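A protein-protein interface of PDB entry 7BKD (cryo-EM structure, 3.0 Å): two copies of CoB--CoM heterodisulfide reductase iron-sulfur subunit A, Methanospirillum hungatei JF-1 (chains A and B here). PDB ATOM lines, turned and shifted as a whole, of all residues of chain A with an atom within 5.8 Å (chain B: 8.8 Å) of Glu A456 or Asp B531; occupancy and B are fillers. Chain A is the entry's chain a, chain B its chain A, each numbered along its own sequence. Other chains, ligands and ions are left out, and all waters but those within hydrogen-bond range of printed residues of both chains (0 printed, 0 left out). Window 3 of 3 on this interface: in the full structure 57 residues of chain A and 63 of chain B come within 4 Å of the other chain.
Lys A452 touches Ser B529 (CE to OG, 3.5 Å).
Lys A452 touches Asp B531 (CD to OD2, 3.9 Å).
NZ of Lys A452 touches CB of Trp B533, 3.9 Å away.
Lys A452 touches Met B534.
OG of Ser B529 touches CE of Met A453, at 3.6 Å.
Pro B414 touches Glu A455 (O to CG, 3.4 Å).
Glu A456 touches Tyr B415 (OE2 to CB, 3.7 Å).
Asn B408 touches Tyr A459.
Hydrophobic or aromatic side chains of chain A that line the printed part of chain B: Met A453 and Tyr A459.
Among the printed residues, Asp or Glu carboxylates within 4 Å of a Lys or Arg side-chain nitrogen of the other chain: Glu A455 with Arg B406 (2.9 Å) and Glu A455 with Arg B448 (3.0 Å).
The side-chain carboxylate (OE1) of Glu A455 lies within salt-bridge range of the guanidinium group (NE) of Arg B406 (2.9 Å).
OE2 of Glu A455 is in salt-bridge range of NH2 of Arg B448, 3.0 Å away.
The side-chain amide nitrogen of Gln B530 sits at hydrogen-bond distance from the side-chain sulfur of Met A453 (3.2 Å).
NZ of Lys A452 lies within hydrogen-bond range of O of Gln B558, 3.2 Å away.
The side-chain sulfur of Met A453 lies close to the side-chain carboxylate of Asp B531 (3.6 Å).
The side-chain carboxylate of Asp B531 lies close to the side-chain carboxylate of Glu A456, at 2.9 Å.
N of Arg B406 sits at hydrogen-bond distance from O of Lys B413 (2.9 Å).
The backbone carbonyl oxygen of Tyr B415 sits at hydrogen-bond distance from the backbone NH of Arg B406, 3.1 Å away.
OH of Tyr B415 sits at hydrogen-bond distance from O of Val B511, at 2.6 Å.
SG of Cys B416 lies close to NH2 of Arg B448 (3.4 Å).
The side-chain hydroxyl (OG) of Ser B529 is in hydrogen-bond range of the side-chain amide oxygen (OE1) of Gln B530, at 3.0 Å.
No position is printed for both chains.
Of the printed residues of chain B, Lys A452 touches Ser B529 (3.5 Å), Asp B531 (3.9 Å), Trp B533 (3.9 Å), Met B534 (3.8 Å) and Gln B558 (3.2 Å).
Of the printed residues of chain B, Met A453 touches Ser B529 (3.6 Å), Gln B530 (3.2 Å) and Asp B531 (3.1 Å).
Printed residues of chain B within 4 Å of Glu A456: Tyr B415 (3.7 Å) and Asp B531 (2.9 Å).
Arg A460 touches none of the printed residues of chain B.
Lys B413 touches none of the printed residues of chain A.
Printed residues of chain A within 4 Å of Pro B414: Glu A455.
Printed residues of chain A within 4 Å of Arg B448: Glu A455.
The nearest printed residue of chain A that does not touch Asp B531 is Gly A451 (5.9 Å).
The nearest printed residue of chain A that does not touch Trp B533 is Met A453 (6.1 Å).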
ATOM      1  N   GLY A 451      31.528  -4.724 -12.688  1.00  0.00           N
ATOM      2  CA  GLY A 451      32.428  -3.864 -11.944  1.00  0.00           C
ATOM      3  C   GLY A 451      32.025  -2.407 -11.937  1.00  0.00           C
ATOM      4  O   GLY A 451      30.893  -2.044 -12.266  1.00  0.00           O
ATOM      5  N   LYS A 452      32.981  -1.556 -11.573  1.00  0.00           N
ATOM      6  CA  LYS A 452      32.740  -0.125 -11.467  1.00  0.00           C
ATOM      7  C   LYS A 452      32.727   0.512 -12.849  1.00  0.00           C
ATOM      8  O   LYS A 452      33.742   0.512 -13.550  1.00  0.00           O
ATOM      9  CB  LYS A 452      33.807   0.527 -10.589  1.00  0.00           C
ATOM     10  CG  LYS A 452      33.753   2.044 -10.558  1.00  0.00           C
ATOM     11  CD  LYS A 452      32.677   2.548  -9.616  1.00  0.00           C
ATOM     12  CE  LYS A 452      32.986   3.949  -9.122  1.00  0.00           C
ATOM     13  NZ  LYS A 452      34.019   3.958  -8.053  1.00  0.00           N
ATOM     14  N   MET A 453      31.571   1.058 -13.228  1.00  0.00           N
ATOM     15  CA  MET A 453      31.277   1.724 -14.494  1.00  0.00           C
ATOM     16  C   MET A 453      31.146   0.727 -15.637  1.00  0.00           C
ATOM     17  O   MET A 453      31.233   1.121 -16.804  1.00  0.00           O
ATOM     18  CB  MET A 453      32.331   2.775 -14.861  1.00  0.00           C
ATOM     19  CG  MET A 453      32.329   3.923 -13.891  1.00  0.00           C
ATOM     20  SD  MET A 453      30.684   4.550 -13.543  1.00  0.00           S
ATOM     21  CE  MET A 453      30.996   5.264 -11.935  1.00  0.00           C
ATOM     22  N   TYR A 454      30.942  -0.553 -15.334  1.00  0.00           N
ATOM     23  CA  TYR A 454      30.824  -1.583 -16.360  1.00  0.00           C
ATOM     24  C   TYR A 454      29.418  -1.621 -16.946  1.00  0.00           C
ATOM     25  O   TYR A 454      29.249  -1.781 -18.159  1.00  0.00           O
ATOM     26  CB  TYR A 454      31.211  -2.931 -15.747  1.00  0.00           C
ATOM     27  CG  TYR A 454      32.702  -3.110 -15.524  1.00  0.00           C
ATOM     28  CD1 TYR A 454      33.412  -4.089 -16.195  1.00  0.00           C
ATOM     29  CD2 TYR A 454      33.416  -2.219 -14.745  1.00  0.00           C
ATOM     30  CE1 TYR A 454      34.770  -4.240 -16.014  1.00  0.00           C
ATOM     31  CE2 TYR A 454      34.772  -2.353 -14.563  1.00  0.00           C
ATOM     32  CZ  TYR A 454      35.447  -3.363 -15.202  1.00  0.00           C
ATOM     33  OH  TYR A 454      36.804  -3.496 -15.025  1.00  0.00           O
ATOM     34  N   GLU A 455      28.399  -1.468 -16.100  1.00  0.00           N
ATOM     35  CA  GLU A 455      27.023  -1.484 -16.585  1.00  0.00           C
ATOM     36  C   GLU A 455      26.718  -0.244 -17.417  1.00  0.00           C
ATOM     37  O   GLU A 455      26.003  -0.323 -18.422  1.00  0.00           O
ATOM     38  CB  GLU A 455      26.056  -1.608 -15.410  1.00  0.00           C
ATOM     39  CG  GLU A 455      24.595  -1.676 -15.804  1.00  0.00           C
ATOM     40  CD  GLU A 455      24.149  -3.090 -16.138  1.00  0.00           C
ATOM     41  OE1 GLU A 455      23.058  -3.253 -16.723  1.00  0.00           O
ATOM     42  OE2 GLU A 455      24.892  -4.040 -15.816  1.00  0.00           O
ATOM     43  N   GLU A 456      27.253   0.910 -17.015  1.00  0.00           N
ATOM     44  CA  GLU A 456      27.076   2.125 -17.805  1.00  0.00           C
ATOM     45  C   GLU A 456      27.766   2.018 -19.158  1.00  0.00           C
ATOM     46  O   GLU A 456      27.271   2.564 -20.150  1.00  0.00           O
ATOM     47  CB  GLU A 456      27.594   3.333 -17.026  1.00  0.00           C
ATOM     48  CG  GLU A 456      26.814   3.638 -15.753  1.00  0.00           C
ATOM     49  CD  GLU A 456      27.189   2.749 -14.577  1.00  0.00           C
ATOM     50  OE1 GLU A 456      27.918   1.754 -14.774  1.00  0.00           O
ATOM     51  OE2 GLU A 456      26.753   3.051 -13.447  1.00  0.00           O
ATOM     52  N   PHE A 457      28.899   1.319 -19.221  1.00  0.00           N
ATOM     53  CA  PHE A 457      29.521   1.031 -20.508  1.00  0.00           C
ATOM     54  C   PHE A 457      28.595   0.195 -21.381  1.00  0.00           C
ATOM     55  O   PHE A 457      28.477   0.436 -22.586  1.00  0.00           O
ATOM     56  CB  PHE A 457      30.853   0.317 -20.285  1.00  0.00           C
ATOM     57  CG  PHE A 457      31.714   0.234 -21.507  1.00  0.00           C
ATOM     58  CD1 PHE A 457      32.277   1.372 -22.053  1.00  0.00           C
ATOM     59  CD2 PHE A 457      31.975  -0.987 -22.103  1.00  0.00           C
ATOM     60  CE1 PHE A 457      33.072   1.293 -23.173  1.00  0.00           C
ATOM     61  CE2 PHE A 457      32.772  -1.072 -23.219  1.00  0.00           C
ATOM     62  CZ  PHE A 457      33.322   0.069 -23.757  1.00  0.00           C
ATOM     63  N   TYR A 458      27.924  -0.787 -20.779  1.00  0.00           N
ATOM     64  CA  TYR A 458      26.950  -1.606 -21.494  1.00  0.00           C
ATOM     65  C   TYR A 458      25.799  -0.755 -22.024  1.00  0.00           C
ATOM     66  O   TYR A 458      25.365  -0.919 -23.173  1.00  0.00           O
ATOM     67  CB  TYR A 458      26.457  -2.697 -20.543  1.00  0.00           C
ATOM     68  CG  TYR A 458      25.377  -3.616 -21.050  1.00  0.00           C
ATOM     69  CD1 TYR A 458      25.344  -4.033 -22.370  1.00  0.00           C
ATOM     70  CD2 TYR A 458      24.404  -4.095 -20.185  1.00  0.00           C
ATOM     71  CE1 TYR A 458      24.358  -4.885 -22.818  1.00  0.00           C
ATOM     72  CE2 TYR A 458      23.419  -4.945 -20.622  1.00  0.00           C
ATOM     73  CZ  TYR A 458      23.399  -5.338 -21.940  1.00  0.00           C
ATOM     74  OH  TYR A 458      22.411  -6.186 -22.376  1.00  0.00           O
ATOM     75  N   TYR A 459      25.309   0.171 -21.200  1.00  0.00           N
ATOM     76  CA  TYR A 459      24.261   1.093 -21.626  1.00  0.00           C
ATOM     77  C   TYR A 459      24.718   1.939 -22.807  1.00  0.00           C
ATOM     78  O   TYR A 459      23.982   2.105 -23.788  1.00  0.00           O
ATOM     79  CB  TYR A 459      23.855   1.976 -20.445  1.00  0.00           C
ATOM     80  CG  TYR A 459      22.520   2.663 -20.587  1.00  0.00           C
ATOM     81  CD1 TYR A 459      22.396   3.828 -21.330  1.00  0.00           C
ATOM     82  CD2 TYR A 459      21.384   2.150 -19.979  1.00  0.00           C
ATOM     83  CE1 TYR A 459      21.180   4.460 -21.460  1.00  0.00           C
ATOM     84  CE2 TYR A 459      20.166   2.776 -20.104  1.00  0.00           C
ATOM     85  CZ  TYR A 459      20.069   3.930 -20.846  1.00  0.00           C
ATOM     86  OH  TYR A 459      18.855   4.560 -20.976  1.00  0.00           O
ATOM     87  N   ARG A 460      25.937   2.475 -22.736  1.00  0.00           N
ATOM     88  CA  ARG A 460      26.462   3.270 -23.841  1.00  0.00           C
ATOM     89  C   ARG A 460      26.579   2.445 -25.115  1.00  0.00           C
ATOM     90  O   ARG A 460      26.250   2.927 -26.205  1.00  0.00           O
ATOM     91  CB  ARG A 460      27.822   3.861 -23.478  1.00  0.00           C
ATOM     92  CG  ARG A 460      27.810   4.868 -22.351  1.00  0.00           C
ATOM     93  CD  ARG A 460      29.222   5.362 -22.078  1.00  0.00           C
ATOM     94  NE  ARG A 460      29.745   6.130 -23.205  1.00  0.00           N
ATOM     95  CZ  ARG A 460      30.713   5.708 -24.012  1.00  0.00           C
ATOM     96  NH1 ARG A 460      31.271   4.523 -23.817  1.00  0.00           N
ATOM     97  NH2 ARG A 460      31.127   6.471 -25.014  1.00  0.00           N
ATOM     98  N   ILE A 461      27.065   1.209 -25.001  1.00  0.00           N
ATOM     99  CA  ILE A 461      27.249   0.382 -26.189  1.00  0.00           C
ATOM    100  C   ILE A 461      25.908   0.081 -26.839  1.00  0.00           C
ATOM    101  O   ILE A 461      25.769   0.147 -28.067  1.00  0.00           O
ATOM    102  CB  ILE A 461      28.015  -0.910 -25.847  1.00  0.00           C
ATOM    103  CG1 ILE A 461      29.411  -0.590 -25.313  1.00  0.00           C
ATOM    104  CG2 ILE A 461      28.141  -1.789 -27.076  1.00  0.00           C
ATOM    105  CD1 ILE A 461      30.083   0.573 -25.994  1.00  0.00           C
ATOM    106  N   ARG B 406      20.704  -1.906 -11.852  1.00  0.00           N
ATOM    107  CA  ARG B 406      20.662  -1.770 -13.330  1.00  0.00           C
ATOM    108  C   ARG B 406      19.368  -1.009 -13.627  1.00  0.00           C
ATOM    109  O   ARG B 406      18.789  -1.249 -14.690  1.00  0.00           O
ATOM    110  CB  ARG B 406      20.825  -3.162 -13.945  1.00  0.00           C
ATOM    111  CG  ARG B 406      21.908  -3.996 -13.277  1.00  0.00           C
ATOM    112  CD  ARG B 406      21.958  -5.430 -13.759  1.00  0.00           C
ATOM    113  NE  ARG B 406      21.986  -5.489 -15.210  1.00  0.00           N
ATOM    114  CZ  ARG B 406      21.725  -6.572 -15.921  1.00  0.00           C
ATOM    115  NH1 ARG B 406      21.414  -7.701 -15.312  1.00  0.00           N
ATOM    116  NH2 ARG B 406      21.778  -6.526 -17.239  1.00  0.00           N
ATOM    117  N   ASP B 407      18.973  -0.087 -12.741  1.00  0.00           N
ATOM    118  CA  ASP B 407      17.705   0.611 -12.887  1.00  0.00           C
ATOM    119  C   ASP B 407      17.973   2.060 -13.262  1.00  0.00           C
ATOM    120  O   ASP B 407      18.708   2.760 -12.560  1.00  0.00           O
ATOM    121  CB  ASP B 407      16.905   0.526 -11.585  1.00  0.00           C
ATOM    122  CG  ASP B 407      15.553   1.196 -11.680  1.00  0.00           C
ATOM    123  OD1 ASP B 407      15.486   2.433 -11.510  1.00  0.00           O
ATOM    124  OD2 ASP B 407      14.552   0.486 -11.902  1.00  0.00           O
ATOM    125  N   ASN B 408      17.381   2.505 -14.366  1.00  0.00           N
ATOM    126  CA  ASN B 408      17.552   3.868 -14.847  1.00  0.00           C
ATOM    127  C   ASN B 408      16.345   4.750 -14.563  1.00  0.00           C
ATOM    128  O   ASN B 408      16.262   5.854 -15.104  1.00  0.00           O
ATOM    129  CB  ASN B 408      17.850   3.863 -16.346  1.00  0.00           C
ATOM    130  CG  ASN B 408      19.182   3.225 -16.672  1.00  0.00           C
ATOM    131  OD1 ASN B 408      19.250   2.047 -17.018  1.00  0.00           O
ATOM    132  ND2 ASN B 408      20.251   4.001 -16.563  1.00  0.00           N
ATOM    133  N   GLY B 412      16.014   3.310  -8.114  1.00  0.00           N
ATOM    134  CA  GLY B 412      17.066   2.380  -7.752  1.00  0.00           C
ATOM    135  C   GLY B 412      18.439   2.868  -8.159  1.00  0.00           C
ATOM    136  O   GLY B 412      18.706   4.070  -8.220  1.00  0.00           O
ATOM    137  N   LYS B 413      19.325   1.920  -8.435  1.00  0.00           N
ATOM    138  CA  LYS B 413      20.677   2.247  -8.848  1.00  0.00           C
ATOM    139  C   LYS B 413      20.929   1.787 -10.277  1.00  0.00           C
ATOM    140  O   LYS B 413      20.453   0.719 -10.676  1.00  0.00           O
ATOM    141  CB  LYS B 413      21.711   1.598  -7.923  1.00  0.00           C
ATOM    142  CG  LYS B 413      21.525   1.938  -6.462  1.00  0.00           C
ATOM    143  CD  LYS B 413      21.738   3.418  -6.218  1.00  0.00           C
ATOM    144  CE  LYS B 413      21.459   3.779  -4.774  1.00  0.00           C
ATOM    145  NZ  LYS B 413      22.218   4.983  -4.353  1.00  0.00           N
ATOM    146  N   PRO B 414      21.668   2.567 -11.068  1.00  0.00           N
ATOM    147  CA  PRO B 414      21.952   2.175 -12.451  1.00  0.00           C
ATOM    148  C   PRO B 414      23.113   1.207 -12.605  1.00  0.00           C
ATOM    149  O   PRO B 414      23.426   0.825 -13.738  1.00  0.00           O
ATOM    150  CB  PRO B 414      22.271   3.518 -13.121  1.00  0.00           C
ATOM    151  CG  PRO B 414      22.834   4.346 -12.032  1.00  0.00           C
ATOM    152  CD  PRO B 414      22.175   3.913 -10.753  1.00  0.00           C
ATOM    153  N   TYR B 415      23.759   0.799 -11.519  1.00  0.00           N
ATOM    154  CA  TYR B 415      24.922  -0.071 -11.586  1.00  0.00           C
ATOM    155  C   TYR B 415      24.580  -1.462 -11.069  1.00  0.00           C
ATOM    156  O   TYR B 415      23.487  -1.720 -10.562  1.00  0.00           O
ATOM    157  CB  TYR B 415      26.094   0.517 -10.792  1.00  0.00           C
ATOM    158  CG  TYR B 415      25.770   0.892  -9.363  1.00  0.00           C
ATOM    159  CD1 TYR B 415      25.561   2.216  -9.005  1.00  0.00           C
ATOM    160  CD2 TYR B 415      25.691  -0.072  -8.370  1.00  0.00           C
ATOM    161  CE1 TYR B 415      25.271   2.566  -7.705  1.00  0.00           C
ATOM    162  CE2 TYR B 415      25.401   0.268  -7.068  1.00  0.00           C
ATOM    163  CZ  TYR B 415      25.192   1.589  -6.739  1.00  0.00           C
ATOM    164  OH  TYR B 415      24.903   1.935  -5.441  1.00  0.00           O
ATOM    165  N   CYS B 416      25.529  -2.374 -11.231  1.00  0.00           N
ATOM    166  CA  CYS B 416      25.344  -3.758 -10.750  1.00  0.00           C
ATOM    167  C   CYS B 416      26.008  -3.818  -9.381  1.00  0.00           C
ATOM    168  O   CYS B 416      27.036  -3.173  -9.215  1.00  0.00           O
ATOM    169  CB  CYS B 416      25.991  -4.716 -11.748  1.00  0.00           C
ATOM    170  SG  CYS B 416      26.221  -6.410 -11.164  1.00  0.00           S
ATOM    171  N   ARG B 448      25.339 -13.679 -12.921  1.00  0.00           N
ATOM    172  CA  ARG B 448      26.709 -13.104 -13.034  1.00  0.00           C
ATOM    173  C   ARG B 448      27.705 -13.802 -12.095  1.00  0.00           C
ATOM    174  O   ARG B 448      27.971 -13.273 -11.018  1.00  0.00           O
ATOM    175  CB  ARG B 448      26.602 -11.586 -12.817  1.00  0.00           C
ATOM    176  CG  ARG B 448      26.071 -10.828 -14.024  1.00  0.00           C
ATOM    177  CD  ARG B 448      26.200  -9.321 -13.964  1.00  0.00           C
ATOM    178  NE  ARG B 448      25.814  -8.758 -15.246  1.00  0.00           N
ATOM    179  CZ  ARG B 448      25.464  -7.498 -15.454  1.00  0.00           C
ATOM    180  NH1 ARG B 448      25.136  -7.094 -16.667  1.00  0.00           N
ATOM    181  NH2 ARG B 448      25.444  -6.645 -14.450  1.00  0.00           N
ATOM    182  N   VAL B 511      23.365  -2.189  -3.129  1.00  0.00           N
ATOM    183  CA  VAL B 511      24.190  -1.665  -2.049  1.00  0.00           C
ATOM    184  C   VAL B 511      24.550  -0.220  -2.364  1.00  0.00           C
ATOM    185  O   VAL B 511      24.717   0.153  -3.530  1.00  0.00           O
ATOM    186  CB  VAL B 511      25.458  -2.512  -1.828  1.00  0.00           C
ATOM    187  CG1 VAL B 511      25.085  -3.894  -1.326  1.00  0.00           C
ATOM    188  CG2 VAL B 511      26.277  -2.601  -3.102  1.00  0.00           C
ATOM    189  N   GLN B 512      24.655   0.588  -1.320  1.00  0.00           N
ATOM    190  CA  GLN B 512      25.007   1.994  -1.420  1.00  0.00           C
ATOM    191  C   GLN B 512      25.957   2.327  -0.281  1.00  0.00           C
ATOM    192  O   GLN B 512      26.056   1.571   0.691  1.00  0.00           O
ATOM    193  CB  GLN B 512      23.759   2.887  -1.365  1.00  0.00           C
ATOM    194  CG  GLN B 512      23.065   2.898  -0.026  1.00  0.00           C
ATOM    195  CD  GLN B 512      21.805   3.731  -0.036  1.00  0.00           C
ATOM    196  OE1 GLN B 512      21.464   4.348  -1.043  1.00  0.00           O
ATOM    197  NE2 GLN B 512      21.104   3.753   1.087  1.00  0.00           N
ATOM    198  N   PRO B 513      26.690   3.436  -0.384  1.00  0.00           N
ATOM    199  CA  PRO B 513      27.588   3.826   0.711  1.00  0.00           C
ATOM    200  C   PRO B 513      26.839   4.017   2.021  1.00  0.00           C
ATOM    201  O   PRO B 513      25.672   4.413   2.043  1.00  0.00           O
ATOM    202  CB  PRO B 513      28.190   5.146   0.219  1.00  0.00           C
ATOM    203  CG  PRO B 513      28.112   5.065  -1.258  1.00  0.00           C
ATOM    204  CD  PRO B 513      26.888   4.269  -1.584  1.00  0.00           C
ATOM    205  N   ASN B 518      29.667  10.108   2.926  1.00  0.00           N
ATOM    206  CA  ASN B 518      29.932  11.266   2.080  1.00  0.00           C
ATOM    207  C   ASN B 518      30.502  12.423   2.888  1.00  0.00           C
ATOM    208  O   ASN B 518      31.415  13.118   2.429  1.00  0.00           O
ATOM    209  CB  ASN B 518      28.658  11.686   1.353  1.00  0.00           C
ATOM    210  CG  ASN B 518      28.503  10.999   0.016  1.00  0.00           C
ATOM    211  OD1 ASN B 518      29.489  10.620  -0.615  1.00  0.00           O
ATOM    212  ND2 ASN B 518      27.262  10.834  -0.426  1.00  0.00           N
ATOM    213  N   ALA B 528      33.704  12.255  -4.805  1.00  0.00           N
ATOM    214  CA  ALA B 528      32.877  11.097  -5.091  1.00  0.00           C
ATOM    215  C   ALA B 528      32.922  10.764  -6.579  1.00  0.00           C
ATOM    216  O   ALA B 528      33.361  11.563  -7.410  1.00  0.00           O
ATOM    217  CB  ALA B 528      31.435  11.340  -4.656  1.00  0.00           C
ATOM    218  N   SER B 529      32.464   9.562  -6.908  1.00  0.00           N
ATOM    219  CA  SER B 529      32.326   9.154  -8.294  1.00  0.00           C
ATOM    220  C   SER B 529      30.898   9.424  -8.760  1.00  0.00           C
ATOM    221  O   SER B 529      30.031   9.829  -7.983  1.00  0.00           O
ATOM    222  CB  SER B 529      32.702   7.683  -8.457  1.00  0.00           C
ATOM    223  OG  SER B 529      32.962   7.376  -9.814  1.00  0.00           O
ATOM    224  N   GLN B 530      30.643   9.208 -10.052  1.00  0.00           N
ATOM    225  CA  GLN B 530      29.311   9.486 -10.582  1.00  0.00           C
ATOM    226  C   GLN B 530      28.302   8.406 -10.196  1.00  0.00           C
ATOM    227  O   GLN B 530      27.094   8.593 -10.376  1.00  0.00           O
ATOM    228  CB  GLN B 530      29.371   9.710 -12.096  1.00  0.00           C
ATOM    229  CG  GLN B 530      29.695   8.512 -12.962  1.00  0.00           C
ATOM    230  CD  GLN B 530      31.192   8.290 -13.086  1.00  0.00           C
ATOM    231  OE1 GLN B 530      31.979   8.819 -12.300  1.00  0.00           O
ATOM    232  NE2 GLN B 530      31.595   7.526 -14.096  1.00  0.00           N
ATOM    233  N   ASP B 531      28.768   7.272  -9.669  1.00  0.00           N
ATOM    234  CA  ASP B 531      27.854   6.375  -8.967  1.00  0.00           C
ATOM    235  C   ASP B 531      27.633   6.763  -7.512  1.00  0.00           C
ATOM    236  O   ASP B 531      26.697   6.251  -6.891  1.00  0.00           O
ATOM    237  CB  ASP B 531      28.338   4.925  -9.012  1.00  0.00           C
ATOM    238  CG  ASP B 531      28.240   4.316 -10.389  1.00  0.00           C
ATOM    239  OD1 ASP B 531      27.422   4.802 -11.198  1.00  0.00           O
ATOM    240  OD2 ASP B 531      28.953   3.325 -10.651  1.00  0.00           O
ATOM    241  N   GLY B 532      28.456   7.647  -6.957  1.00  0.00           N
ATOM    242  CA  GLY B 532      28.358   8.022  -5.564  1.00  0.00           C
ATOM    243  C   GLY B 532      29.396   7.392  -4.662  1.00  0.00           C
ATOM    244  O   GLY B 532      29.483   7.772  -3.489  1.00  0.00           O
ATOM    245  N   TRP B 533      30.175   6.442  -5.166  1.00  0.00           N
ATOM    246  CA  TRP B 533      31.281   5.889  -4.405  1.00  0.00           C
ATOM    247  C   TRP B 533      32.478   6.838  -4.459  1.00  0.00           C
ATOM    248  O   TRP B 533      32.517   7.789  -5.244  1.00  0.00           O
ATOM    249  CB  TRP B 533      31.663   4.510  -4.940  1.00  0.00           C
ATOM    250  CG  TRP B 533      30.497   3.587  -5.104  1.00  0.00           C
ATOM    251  CD1 TRP B 533      29.797   3.351  -6.248  1.00  0.00           C
ATOM    252  CD2 TRP B 533      29.895   2.773  -4.092  1.00  0.00           C
ATOM    253  NE1 TRP B 533      28.796   2.443  -6.013  1.00  0.00           N
ATOM    254  CE2 TRP B 533      28.835   2.073  -4.695  1.00  0.00           C
ATOM    255  CE3 TRP B 533      30.150   2.568  -2.734  1.00  0.00           C
ATOM    256  CZ2 TRP B 533      28.030   1.185  -3.989  1.00  0.00           C
ATOM    257  CZ3 TRP B 533      29.351   1.686  -2.035  1.00  0.00           C
ATOM    258  CH2 TRP B 533      28.304   1.006  -2.663  1.00  0.00           C
ATOM    259  N   MET B 534      33.462   6.577  -3.605  1.00  0.00           N
ATOM    260  CA  MET B 534      34.660   7.404  -3.582  1.00  0.00           C
ATOM    261  C   MET B 534      35.451   7.239  -4.874  1.00  0.00           C
ATOM    262  O   MET B 534      35.577   6.134  -5.408  1.00  0.00           O
ATOM    263  CB  MET B 534      35.525   7.054  -2.373  1.00  0.00           C
ATOM    264  CG  MET B 534      34.865   7.372  -1.043  1.00  0.00           C
ATOM    265  SD  MET B 534      35.617   6.530   0.360  1.00  0.00           S
ATOM    266  CE  MET B 534      34.482   6.974   1.670  1.00  0.00           C
ATOM    267  N   LEU B 535      35.971   8.352  -5.382  1.00  0.00           N
ATOM    268  CA  LEU B 535      36.680   8.359  -6.653  1.00  0.00           C
ATOM    269  C   LEU B 535      38.137   7.952  -6.469  1.00  0.00           C
ATOM    270  O   LEU B 535      38.722   8.118  -5.396  1.00  0.00           O
ATOM    271  CB  LEU B 535      36.602   9.742  -7.299  1.00  0.00           C
ATOM    272  CG  LEU B 535      36.977   9.820  -8.777  1.00  0.00           C
ATOM    273  CD1 LEU B 535      36.266   8.733  -9.562  1.00  0.00           C
ATOM    274  CD2 LEU B 535      36.657  11.191  -9.339  1.00  0.00           C
ATOM    275  N   GLN B 558      35.066   1.960  -1.990  1.00  0.00           N
ATOM    276  CA  GLN B 558      35.511   2.274  -3.339  1.00  0.00           C
ATOM    277  C   GLN B 558      34.588   1.705  -4.411  1.00  0.00           C
ATOM    278  O   GLN B 558      34.687   2.111  -5.574  1.00  0.00           O
ATOM    279  CB  GLN B 558      36.936   1.747  -3.532  1.00  0.00           C
ATOM    280  CG  GLN B 558      37.632   2.219  -4.786  1.00  0.00           C
ATOM    281  CD  GLN B 558      37.693   1.134  -5.838  1.00  0.00           C
ATOM    282  OE1 GLN B 558      37.883  -0.035  -5.519  1.00  0.00           O
ATOM    283  NE2 GLN B 558      37.522   1.512  -7.094  1.00  0.00           N
ATOM    284  N   GLY B 559      33.686   0.802  -4.046  1.00  0.00           N
ATOM    285  CA  GLY B 559      32.828   0.135  -4.996  1.00  0.00           C
ATOM    286  C   GLY B 559      32.573  -1.294  -4.566  1.00  0.00           C
ATOM    287  O   GLY B 559      33.448  -1.952  -3.999  1.00  0.00           O
ATOM    288  N   PRO B 560      31.368  -1.800  -4.824  1.00  0.00           N
ATOM    289  CA  PRO B 560      31.009  -3.140  -4.338  1.00  0.00           C
ATOM    290  C   PRO B 560      31.978  -4.205  -4.831  1.00  0.00           C
ATOM    291  O   PRO B 560      32.382  -4.215  -5.995  1.00  0.00           O
ATOM    292  CB  PRO B 560      29.599  -3.356  -4.899  1.00  0.00           C
ATOM    293  CG  PRO B 560      29.414  -2.299  -5.946  1.00  0.00           C
ATOM    294  CD  PRO B 560      30.251  -1.147  -5.522  1.00  0.00           C
